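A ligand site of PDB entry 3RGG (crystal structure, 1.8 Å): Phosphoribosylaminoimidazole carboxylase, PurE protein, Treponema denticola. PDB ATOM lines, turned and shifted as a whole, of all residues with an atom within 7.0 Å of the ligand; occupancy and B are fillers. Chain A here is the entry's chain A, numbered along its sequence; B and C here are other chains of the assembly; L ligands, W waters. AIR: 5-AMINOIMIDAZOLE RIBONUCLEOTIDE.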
ATOM      1  N   MET A   9      -7.978  14.477   6.252  1.00  0.00           N
ATOM      2  CA  MET A   9      -8.053  13.415   5.225  1.00  0.00           C
ATOM      3  C   MET A   9      -8.209  13.942   3.799  1.00  0.00           C
ATOM      4  O   MET A   9      -8.770  15.044   3.563  1.00  0.00           O
ATOM      5  CB  MET A   9      -9.182  12.426   5.543  1.00  0.00           C
ATOM      6  CG  MET A   9     -10.558  12.961   5.279  1.00  0.00           C
ATOM      7  SD  MET A   9     -11.836  12.037   6.169  1.00  0.00           S
ATOM      8  CE  MET A   9     -11.750  12.828   7.789  1.00  0.00           C
ATOM      9  N   GLY A  10      -7.774  13.139   2.850  1.00  0.00           N
ATOM     10  CA  GLY A  10      -7.865  13.478   1.424  1.00  0.00           C
ATOM     11  C   GLY A  10      -9.224  13.396   0.737  1.00  0.00           C
ATOM     12  O   GLY A  10      -9.463  14.101  -0.245  1.00  0.00           O
ATOM     13  N   SER A  11     -10.105  12.532   1.240  1.00  0.00           N
ATOM     14  CA  SER A  11     -11.396  12.304   0.637  1.00  0.00           C
ATOM     15  C   SER A  11     -12.412  11.882   1.733  1.00  0.00           C
ATOM     16  O   SER A  11     -12.050  11.218   2.711  1.00  0.00           O
ATOM     17  CB  SER A  11     -11.344  11.180  -0.419  1.00  0.00           C
ATOM     18  OG  SER A  11     -12.663  10.726  -0.759  1.00  0.00           O
ATOM     19  N   SER A  12     -13.665  12.240   1.531  1.00  0.00           N
ATOM     20  CA  SER A  12     -14.733  11.735   2.400  1.00  0.00           C
ATOM     21  C   SER A  12     -14.746  10.193   2.492  1.00  0.00           C
ATOM     22  O   SER A  12     -15.182   9.636   3.487  1.00  0.00           O
ATOM     23  CB  SER A  12     -16.119  12.279   1.978  1.00  0.00           C
ATOM     24  OG  SER A  12     -16.640  11.576   0.865  1.00  0.00           O
ATOM     25  N   SER A  13     -14.220   9.501   1.485  1.00  0.00           N
ATOM     26  CA  SER A  13     -14.198   8.035   1.536  1.00  0.00           C
ATOM     27  C   SER A  13     -13.238   7.503   2.646  1.00  0.00           C
ATOM     28  O   SER A  13     -13.424   6.391   3.161  1.00  0.00           O
ATOM     29  CB  SER A  13     -13.915   7.444   0.135  1.00  0.00           C
ATOM     30  OG  SER A  13     -12.553   7.659  -0.229  1.00  0.00           O
ATOM     31  N   ASP A  14     -12.322   8.365   3.116  1.00  0.00           N
ATOM     32  CA  ASP A  14     -11.445   8.072   4.286  1.00  0.00           C
ATOM     33  C   ASP A  14     -12.089   8.222   5.692  1.00  0.00           C
ATOM     34  O   ASP A  14     -11.433   8.008   6.722  1.00  0.00           O
ATOM     35  CB  ASP A  14     -10.235   9.029   4.263  1.00  0.00           C
ATOM     36  CG  ASP A  14      -9.418   8.964   2.965  1.00  0.00           C
ATOM     37  OD1 ASP A  14      -9.235   7.836   2.439  1.00  0.00           O
ATOM     38  OD2 ASP A  14      -8.906  10.032   2.510  1.00  0.00           O
ATOM     39  N   GLY A  37      -9.501  17.613   2.639  1.00  0.00           N
ATOM     40  CA  GLY A  37      -8.846  18.365   1.585  1.00  0.00           C
ATOM     41  C   GLY A  37      -7.785  17.490   0.944  1.00  0.00           C
ATOM     42  O   GLY A  37      -7.090  16.746   1.634  1.00  0.00           O
ATOM     43  N   SER A  38      -7.640  17.630  -0.378  1.00  0.00           N
ATOM     44  CA  SER A  38      -6.774  16.802  -1.170  1.00  0.00           C
ATOM     45  C   SER A  38      -5.591  17.649  -1.585  1.00  0.00           C
ATOM     46  O   SER A  38      -5.774  18.759  -2.024  1.00  0.00           O
ATOM     47  CB  SER A  38      -7.513  16.351  -2.434  1.00  0.00           C
ATOM     48  OG  SER A  38      -6.568  15.867  -3.362  1.00  0.00           O
ATOM     49  N   ALA A  39      -4.384  17.084  -1.467  1.00  0.00           N
ATOM     50  CA  ALA A  39      -3.174  17.702  -1.995  1.00  0.00           C
ATOM     51  C   ALA A  39      -3.110  17.706  -3.525  1.00  0.00           C
ATOM     52  O   ALA A  39      -2.413  18.559  -4.096  1.00  0.00           O
ATOM     53  CB  ALA A  39      -1.886  17.009  -1.427  1.00  0.00           C
ATOM     54  N   HIS A  40      -3.811  16.801  -4.187  1.00  0.00           N
ATOM     55  CA  HIS A  40      -3.859  16.828  -5.649  1.00  0.00           C
ATOM     56  C   HIS A  40      -4.911  17.821  -6.195  1.00  0.00           C
ATOM     57  O   HIS A  40      -4.604  18.642  -7.074  1.00  0.00           O
ATOM     58  CB  HIS A  40      -4.170  15.447  -6.229  1.00  0.00           C
ATOM     59  CG  HIS A  40      -3.120  14.406  -5.967  1.00  0.00           C
ATOM     60  ND1 HIS A  40      -3.285  13.106  -6.381  1.00  0.00           N
ATOM     61  CD2 HIS A  40      -1.881  14.464  -5.428  1.00  0.00           C
ATOM     62  CE1 HIS A  40      -2.215  12.399  -6.072  1.00  0.00           C
ATOM     63  NE2 HIS A  40      -1.335  13.193  -5.500  1.00  0.00           N
ATOM     64  N   LYS A  41      -6.151  17.743  -5.691  1.00  0.00           N
ATOM     65  CA  LYS A  41      -7.294  18.418  -6.345  1.00  0.00           C
ATOM     66  C   LYS A  41      -7.651  19.768  -5.720  1.00  0.00           C
ATOM     67  O   LYS A  41      -8.309  20.576  -6.358  1.00  0.00           O
ATOM     68  CB  LYS A  41      -8.539  17.490  -6.322  1.00  0.00           C
ATOM     69  CG  LYS A  41      -8.434  16.326  -7.270  1.00  0.00           C
ATOM     70  CD  LYS A  41      -9.669  15.387  -7.197  1.00  0.00           C
ATOM     71  CE  LYS A  41      -9.530  14.318  -6.156  1.00  0.00           C
ATOM     72  NZ  LYS A  41     -10.570  13.259  -6.328  1.00  0.00           N
ATOM     73  N   ILE A  65      -4.228  11.534   6.528  1.00  0.00           N
ATOM     74  CA  ILE A  65      -4.818  10.319   5.995  1.00  0.00           C
ATOM     75  C   ILE A  65      -5.063  10.516   4.501  1.00  0.00           C
ATOM     76  O   ILE A  65      -5.927  11.297   4.107  1.00  0.00           O
ATOM     77  CB  ILE A  65      -6.178  10.048   6.629  1.00  0.00           C
ATOM     78  CG1 ILE A  65      -6.079   9.911   8.168  1.00  0.00           C
ATOM     79  CG2 ILE A  65      -6.870   8.803   6.009  1.00  0.00           C
ATOM     80  CD1 ILE A  65      -7.492   9.976   8.857  1.00  0.00           C
ATOM     81  N   ALA A  66      -4.346   9.780   3.683  1.00  0.00           N
ATOM     82  CA  ALA A  66      -4.671   9.756   2.253  1.00  0.00           C
ATOM     83  C   ALA A  66      -4.341   8.379   1.748  1.00  0.00           C
ATOM     84  O   ALA A  66      -3.231   7.828   2.025  1.00  0.00           O
ATOM     85  CB  ALA A  66      -3.908  10.818   1.505  1.00  0.00           C
ATOM     86  N   GLY A  67      -5.305   7.820   1.021  1.00  0.00           N
ATOM     87  CA  GLY A  67      -5.088   6.516   0.414  1.00  0.00           C
ATOM     88  C   GLY A  67      -4.325   6.646  -0.903  1.00  0.00           C
ATOM     89  O   GLY A  67      -3.993   7.750  -1.334  1.00  0.00           O
ATOM     90  N   ARG A  68      -4.026   5.513  -1.541  1.00  0.00           N
ATOM     91  CA  ARG A  68      -3.321   5.531  -2.826  1.00  0.00           C
ATOM     92  C   ARG A  68      -1.999   6.245  -2.659  1.00  0.00           C
ATOM     93  O   ARG A  68      -1.351   6.064  -1.633  1.00  0.00           O
ATOM     94  CB  ARG A  68      -4.220   6.118  -3.943  1.00  0.00           C
ATOM     95  CG  ARG A  68      -5.593   5.478  -3.950  1.00  0.00           C
ATOM     96  CD  ARG A  68      -6.393   5.872  -5.181  1.00  0.00           C
ATOM     97  NE  ARG A  68      -7.655   5.118  -5.254  1.00  0.00           N
ATOM     98  CZ  ARG A  68      -8.449   5.088  -6.297  1.00  0.00           C
ATOM     99  NH1 ARG A  68      -8.196   5.824  -7.374  1.00  0.00           N
ATOM    100  NH2 ARG A  68      -9.575   4.358  -6.260  1.00  0.00           N
ATOM    101  N   SER A  69      -1.559   7.012  -3.658  1.00  0.00           N
ATOM    102  CA  SER A  69      -0.293   7.726  -3.522  1.00  0.00           C
ATOM    103  C   SER A  69      -0.494   8.899  -2.560  1.00  0.00           C
ATOM    104  O   SER A  69      -1.186   9.845  -2.878  1.00  0.00           O
ATOM    105  CB  SER A  69       0.203   8.257  -4.844  1.00  0.00           C
ATOM    106  OG  SER A  69       1.388   9.034  -4.621  1.00  0.00           O
ATOM    107  N   ASN A  70       0.122   8.794  -1.388  1.00  0.00           N
ATOM    108  CA  ASN A  70      -0.054   9.771  -0.312  1.00  0.00           C
ATOM    109  C   ASN A  70       0.859  10.972  -0.525  1.00  0.00           C
ATOM    110  O   ASN A  70       2.004  11.016  -0.102  1.00  0.00           O
ATOM    111  CB  ASN A  70       0.231   9.104   1.033  1.00  0.00           C
ATOM    112  CG  ASN A  70       0.065  10.059   2.199  1.00  0.00           C
ATOM    113  OD1 ASN A  70      -0.366  11.207   2.024  1.00  0.00           O
ATOM    114  ND2 ASN A  70       0.432   9.608   3.390  1.00  0.00           N
ATOM    115  N   ALA A  71       0.314  11.978  -1.190  1.00  0.00           N
ATOM    116  CA  ALA A  71       0.965  13.278  -1.347  1.00  0.00           C
ATOM    117  C   ALA A  71       0.674  14.179  -0.125  1.00  0.00           C
ATOM    118  O   ALA A  71       1.442  15.098   0.175  1.00  0.00           O
ATOM    119  CB  ALA A  71       0.416  13.960  -2.626  1.00  0.00           C
ATOM    120  N   LEU A  72      -0.432  13.889   0.570  1.00  0.00           N
ATOM    121  CA  LEU A  72      -0.962  14.728   1.617  1.00  0.00           C
ATOM    122  C   LEU A  72      -0.026  14.835   2.802  1.00  0.00           C
ATOM    123  O   LEU A  72       0.283  15.963   3.235  1.00  0.00           O
ATOM    124  CB  LEU A  72      -2.336  14.205   2.075  1.00  0.00           C
ATOM    125  CG  LEU A  72      -3.091  15.097   3.073  1.00  0.00           C
ATOM    126  CD1 LEU A  72      -3.309  16.543   2.565  1.00  0.00           C
ATOM    127  CD2 LEU A  72      -4.413  14.445   3.395  1.00  0.00           C
ATOM    128  N   PRO A  89      -5.077   4.955   5.152  1.00  0.00           N
ATOM    129  CA  PRO A  89      -6.029   3.872   5.240  1.00  0.00           C
ATOM    130  C   PRO A  89      -5.423   2.552   4.657  1.00  0.00           C
ATOM    131  O   PRO A  89      -4.452   2.579   3.843  1.00  0.00           O
ATOM    132  CB  PRO A  89      -7.211   4.386   4.421  1.00  0.00           C
ATOM    133  CG  PRO A  89      -6.588   5.259   3.388  1.00  0.00           C
ATOM    134  CD  PRO A  89      -5.408   5.907   4.073  1.00  0.00           C
ATOM    135  N   ARG B 104      -0.540   5.482  -8.608  1.00  0.00           N
ATOM    136  CA  ARG B 104      -1.812   5.305  -7.878  1.00  0.00           C
ATOM    137  C   ARG B 104      -2.492   6.652  -7.557  1.00  0.00           C
ATOM    138  O   ARG B 104      -2.391   7.175  -6.438  1.00  0.00           O
ATOM    139  CB  ARG B 104      -1.546   4.510  -6.607  1.00  0.00           C
ATOM    140  CG  ARG B 104      -1.420   3.023  -6.926  1.00  0.00           C
ATOM    141  CD  ARG B 104      -2.758   2.362  -6.925  1.00  0.00           C
ATOM    142  NE  ARG B 104      -3.361   2.213  -5.595  1.00  0.00           N
ATOM    143  CZ  ARG B 104      -4.637   1.912  -5.323  1.00  0.00           C
ATOM    144  NH1 ARG B 104      -5.574   1.813  -6.256  1.00  0.00           N
ATOM    145  NH2 ARG B 104      -4.995   1.679  -4.049  1.00  0.00           N
ATOM    146  N   MET B 105      -3.152   7.190  -8.573  1.00  0.00           N
ATOM    147  CA  MET B 105      -3.857   8.460  -8.482  1.00  0.00           C
ATOM    148  C   MET B 105      -5.282   8.318  -8.039  1.00  0.00           C
ATOM    149  O   MET B 105      -5.946   7.308  -8.316  1.00  0.00           O
ATOM    150  CB  MET B 105      -3.821   9.148  -9.855  1.00  0.00           C
ATOM    151  CG  MET B 105      -2.390   9.429 -10.345  1.00  0.00           C
ATOM    152  SD  MET B 105      -1.472  10.597  -9.352  1.00  0.00           S
ATOM    153  CE  MET B 105      -0.392   9.561  -8.342  1.00  0.00           C
ATOM    154  N   PRO B 106      -5.789   9.348  -7.332  1.00  0.00           N
ATOM    155  CA  PRO B 106      -7.189   9.370  -7.012  1.00  0.00           C
ATOM    156  C   PRO B 106      -8.025   9.644  -8.271  1.00  0.00           C
ATOM    157  O   PRO B 106      -7.453   9.871  -9.348  1.00  0.00           O
ATOM    158  CB  PRO B 106      -7.297  10.531  -6.034  1.00  0.00           C
ATOM    159  CG  PRO B 106      -6.206  11.443  -6.473  1.00  0.00           C
ATOM    160  CD  PRO B 106      -5.088  10.584  -6.907  1.00  0.00           C
ATOM    161  N   SER B 107      -9.337   9.575  -8.135  1.00  0.00           N
ATOM    162  CA  SER B 107     -10.226   9.963  -9.243  1.00  0.00           C
ATOM    163  C   SER B 107      -9.982  11.416  -9.635  1.00  0.00           C
ATOM    164  O   SER B 107      -9.741  12.259  -8.764  1.00  0.00           O
ATOM    165  CB  SER B 107     -11.715   9.797  -8.864  1.00  0.00           C
ATOM    166  OG  SER B 107     -12.068  10.588  -7.735  1.00  0.00           O
ATOM    167  N   GLY B 108      -9.998  11.706 -10.928  1.00  0.00           N
ATOM    168  CA  GLY B 108      -9.891  13.083 -11.421  1.00  0.00           C
ATOM    169  C   GLY B 108      -8.497  13.603 -11.602  1.00  0.00           C
ATOM    170  O   GLY B 108      -8.327  14.777 -11.834  1.00  0.00           O
ATOM    171  N   ILE B 109      -7.479  12.741 -11.479  1.00  0.00           N
ATOM    172  CA  ILE B 109      -6.057  13.129 -11.577  1.00  0.00           C
ATOM    173  C   ILE B 109      -5.461  12.133 -12.570  1.00  0.00           C
ATOM    174  O   ILE B 109      -5.550  10.911 -12.357  1.00  0.00           O
ATOM    175  CB  ILE B 109      -5.332  13.036 -10.192  1.00  0.00           C
ATOM    176  CG1 ILE B 109      -5.963  14.016  -9.213  1.00  0.00           C
ATOM    177  CG2 ILE B 109      -3.824  13.279 -10.273  1.00  0.00           C
ATOM    178  CD1 ILE B 109      -5.696  15.520  -9.527  1.00  0.00           C
ATOM    179  N   LYS C 149     -16.641  19.484  -4.844  1.00  0.00           N
ATOM    180  CA  LYS C 149     -17.226  18.433  -4.014  1.00  0.00           C
ATOM    181  C   LYS C 149     -16.389  18.219  -2.755  1.00  0.00           C
ATOM    182  O   LYS C 149     -16.912  18.042  -1.666  1.00  0.00           O
ATOM    183  CB  LYS C 149     -17.332  17.112  -4.801  1.00  0.00           C
ATOM    184  CG  LYS C 149     -17.792  15.886  -3.992  1.00  0.00           C
ATOM    185  CD  LYS C 149     -17.406  14.588  -4.690  1.00  0.00           C
ATOM    186  CE  LYS C 149     -17.973  13.318  -3.970  1.00  0.00           C
ATOM    187  NZ  LYS C 149     -17.887  13.325  -2.455  1.00  0.00           N
ATOM    188  N   ILE C 150     -15.068  18.241  -2.902  1.00  0.00           N
ATOM    189  CA  ILE C 150     -14.182  18.054  -1.762  1.00  0.00           C
ATOM    190  C   ILE C 150     -14.362  19.174  -0.736  1.00  0.00           C
ATOM    191  O   ILE C 150     -14.500  18.926   0.469  1.00  0.00           O
ATOM    192  CB  ILE C 150     -12.719  17.989  -2.215  1.00  0.00           C
ATOM    193  CG1 ILE C 150     -12.442  16.660  -2.904  1.00  0.00           C
ATOM    194  CG2 ILE C 150     -11.794  18.139  -1.043  1.00  0.00           C
ATOM    195  CD1 ILE C 150     -11.095  16.648  -3.660  1.00  0.00           C
HETATM  196  N1  AIR L   1      -6.160  10.981  -2.397  1.00  0.00           N
HETATM  197  C2  AIR L   1      -6.841  12.170  -2.517  1.00  0.00           C
HETATM  198  N3  AIR L   1      -6.035  13.136  -3.023  1.00  0.00           N
HETATM  199  C4  AIR L   1      -4.821  12.571  -3.247  1.00  0.00           C
HETATM  200  C5  AIR L   1      -4.927  11.240  -2.823  1.00  0.00           C
HETATM  201  N6  AIR L   1      -3.917  10.309  -2.855  1.00  0.00           N
HETATM  202  C1' AIR L   1      -6.618   9.690  -1.869  1.00  0.00           C
HETATM  203  C2' AIR L   1      -7.794   9.815  -0.922  1.00  0.00           C
HETATM  204  C3' AIR L   1      -8.462   8.440  -1.038  1.00  0.00           C
HETATM  205  C4' AIR L   1      -8.104   7.998  -2.450  1.00  0.00           C
HETATM  206  O4' AIR L   1      -7.016   8.796  -2.934  1.00  0.00           O
HETATM  207  O2' AIR L   1      -7.365  10.105   0.377  1.00  0.00           O
HETATM  208  O3' AIR L   1      -7.998   7.566   0.019  1.00  0.00           O
HETATM  209  C5' AIR L   1      -9.239   8.265  -3.420  1.00  0.00           C
HETATM  210  O5' AIR L   1      -9.555   9.681  -3.401  1.00  0.00           O
HETATM  211  P   AIR L   1     -10.892  10.178  -4.200  1.00  0.00           P
HETATM  212  O6  AIR L   1     -10.774   9.454  -5.529  1.00  0.00           O
HETATM  213  O7  AIR L   1     -10.711  11.681  -4.259  1.00  0.00           O
HETATM  214  O8  AIR L   1     -11.999   9.718  -3.279  1.00  0.00           O
HETATM  215  O   HOH W   1     -10.636  13.714  -2.550  1.00  0.00           O
HETATM  216  O   HOH W   2      -4.502  14.116  -0.988  1.00  0.00           O
HETATM  217  O   HOH W   3      -2.553  12.211  -1.303  1.00  0.00           O
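O6 of the ligand sits at hydrogen-bond distance from OG of Ser 107 of chain B, 2.8 Å away.
The side-chain hydroxyl (OG) of Ser 38 sits at hydrogen-bond distance from a nitrogen (N3) of the ligand, at 2.8 Å.
The side-chain hydroxyl (OG) of Ser 11 sits at hydrogen-bond distance from an oxygen (O8) of the ligand (2.8 Å).
O7 of the ligand is in salt-bridge range of NZ of Lys 41.
O of Ser 69 is in hydrogen-bond range of N6 of the ligand (2.8 Å).
The backbone NH (N) of Gly 67 is in hydrogen-bond range of an oxygen (O3') of the ligand (2.9 Å).
The backbone NH of Ser 107 of chain B is in hydrogen-bond range of an oxygen (O6) of the ligand, 3.0 Å away.
The backbone carbonyl oxygen (O) of Gly 67 sits at hydrogen-bond distance from a nitrogen (N6) of the ligand (3.0 Å).
The side-chain carboxylate of Asp 14 sits at hydrogen-bond distance from an oxygen (O2') of the ligand.
The backbone carbonyl oxygen (O) of Met 105 of chain B sits at hydrogen-bond distance from the guanidinium group (NH1) of Arg 68, 2.9 Å away.
The backbone NH (N) of Gly 10 sits at hydrogen-bond distance from the side-chain carboxylate (OD2) of Asp 14.
The backbone NH (N) of Gly 10 sits at hydrogen-bond distance from the backbone carbonyl oxygen (O) of Ile 65 (2.9 Å).
OG of Ser 11 sits at hydrogen-bond distance from N of Ser 13, at 3.0 Å.
OD2 of Asp 14 sits at hydrogen-bond distance from N of Ser 11 (3.0 Å).
OG of Ser 38 is in hydrogen-bond range of N of His 40.
N of Lys 41 sits at hydrogen-bond distance from OG of Ser 38.
NZ of Lys 41 is in hydrogen-bond range of O of Ser 107 of chain B (2.8 Å).
CA of Gly 10 touches O2' of the ligand, at 3.6 Å.
Ser 13 touches the ligand.
ND1 of His 40 touches C4 of the ligand, at 3.5 Å.
Ala 66 touches the ligand.
Arg 68 touches the ligand (CD to O4', 3.7 Å).
CB of Pro 106 of chain B touches O4' of the ligand, at 3.6 Å.
Hydrophobic or aromatic side chains that line the ligand: His 40, Ala 66 and Pro 106 of chain B.
Water W1 bridges the backbone carbonyl oxygen (O) of Gly 10 (2.6 Å) and an oxygen (O7) of the ligand (2.7 Å).
Water W2 bridges a nitrogen (N3) of the ligand and the backbone NH (N) of Ala 39.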
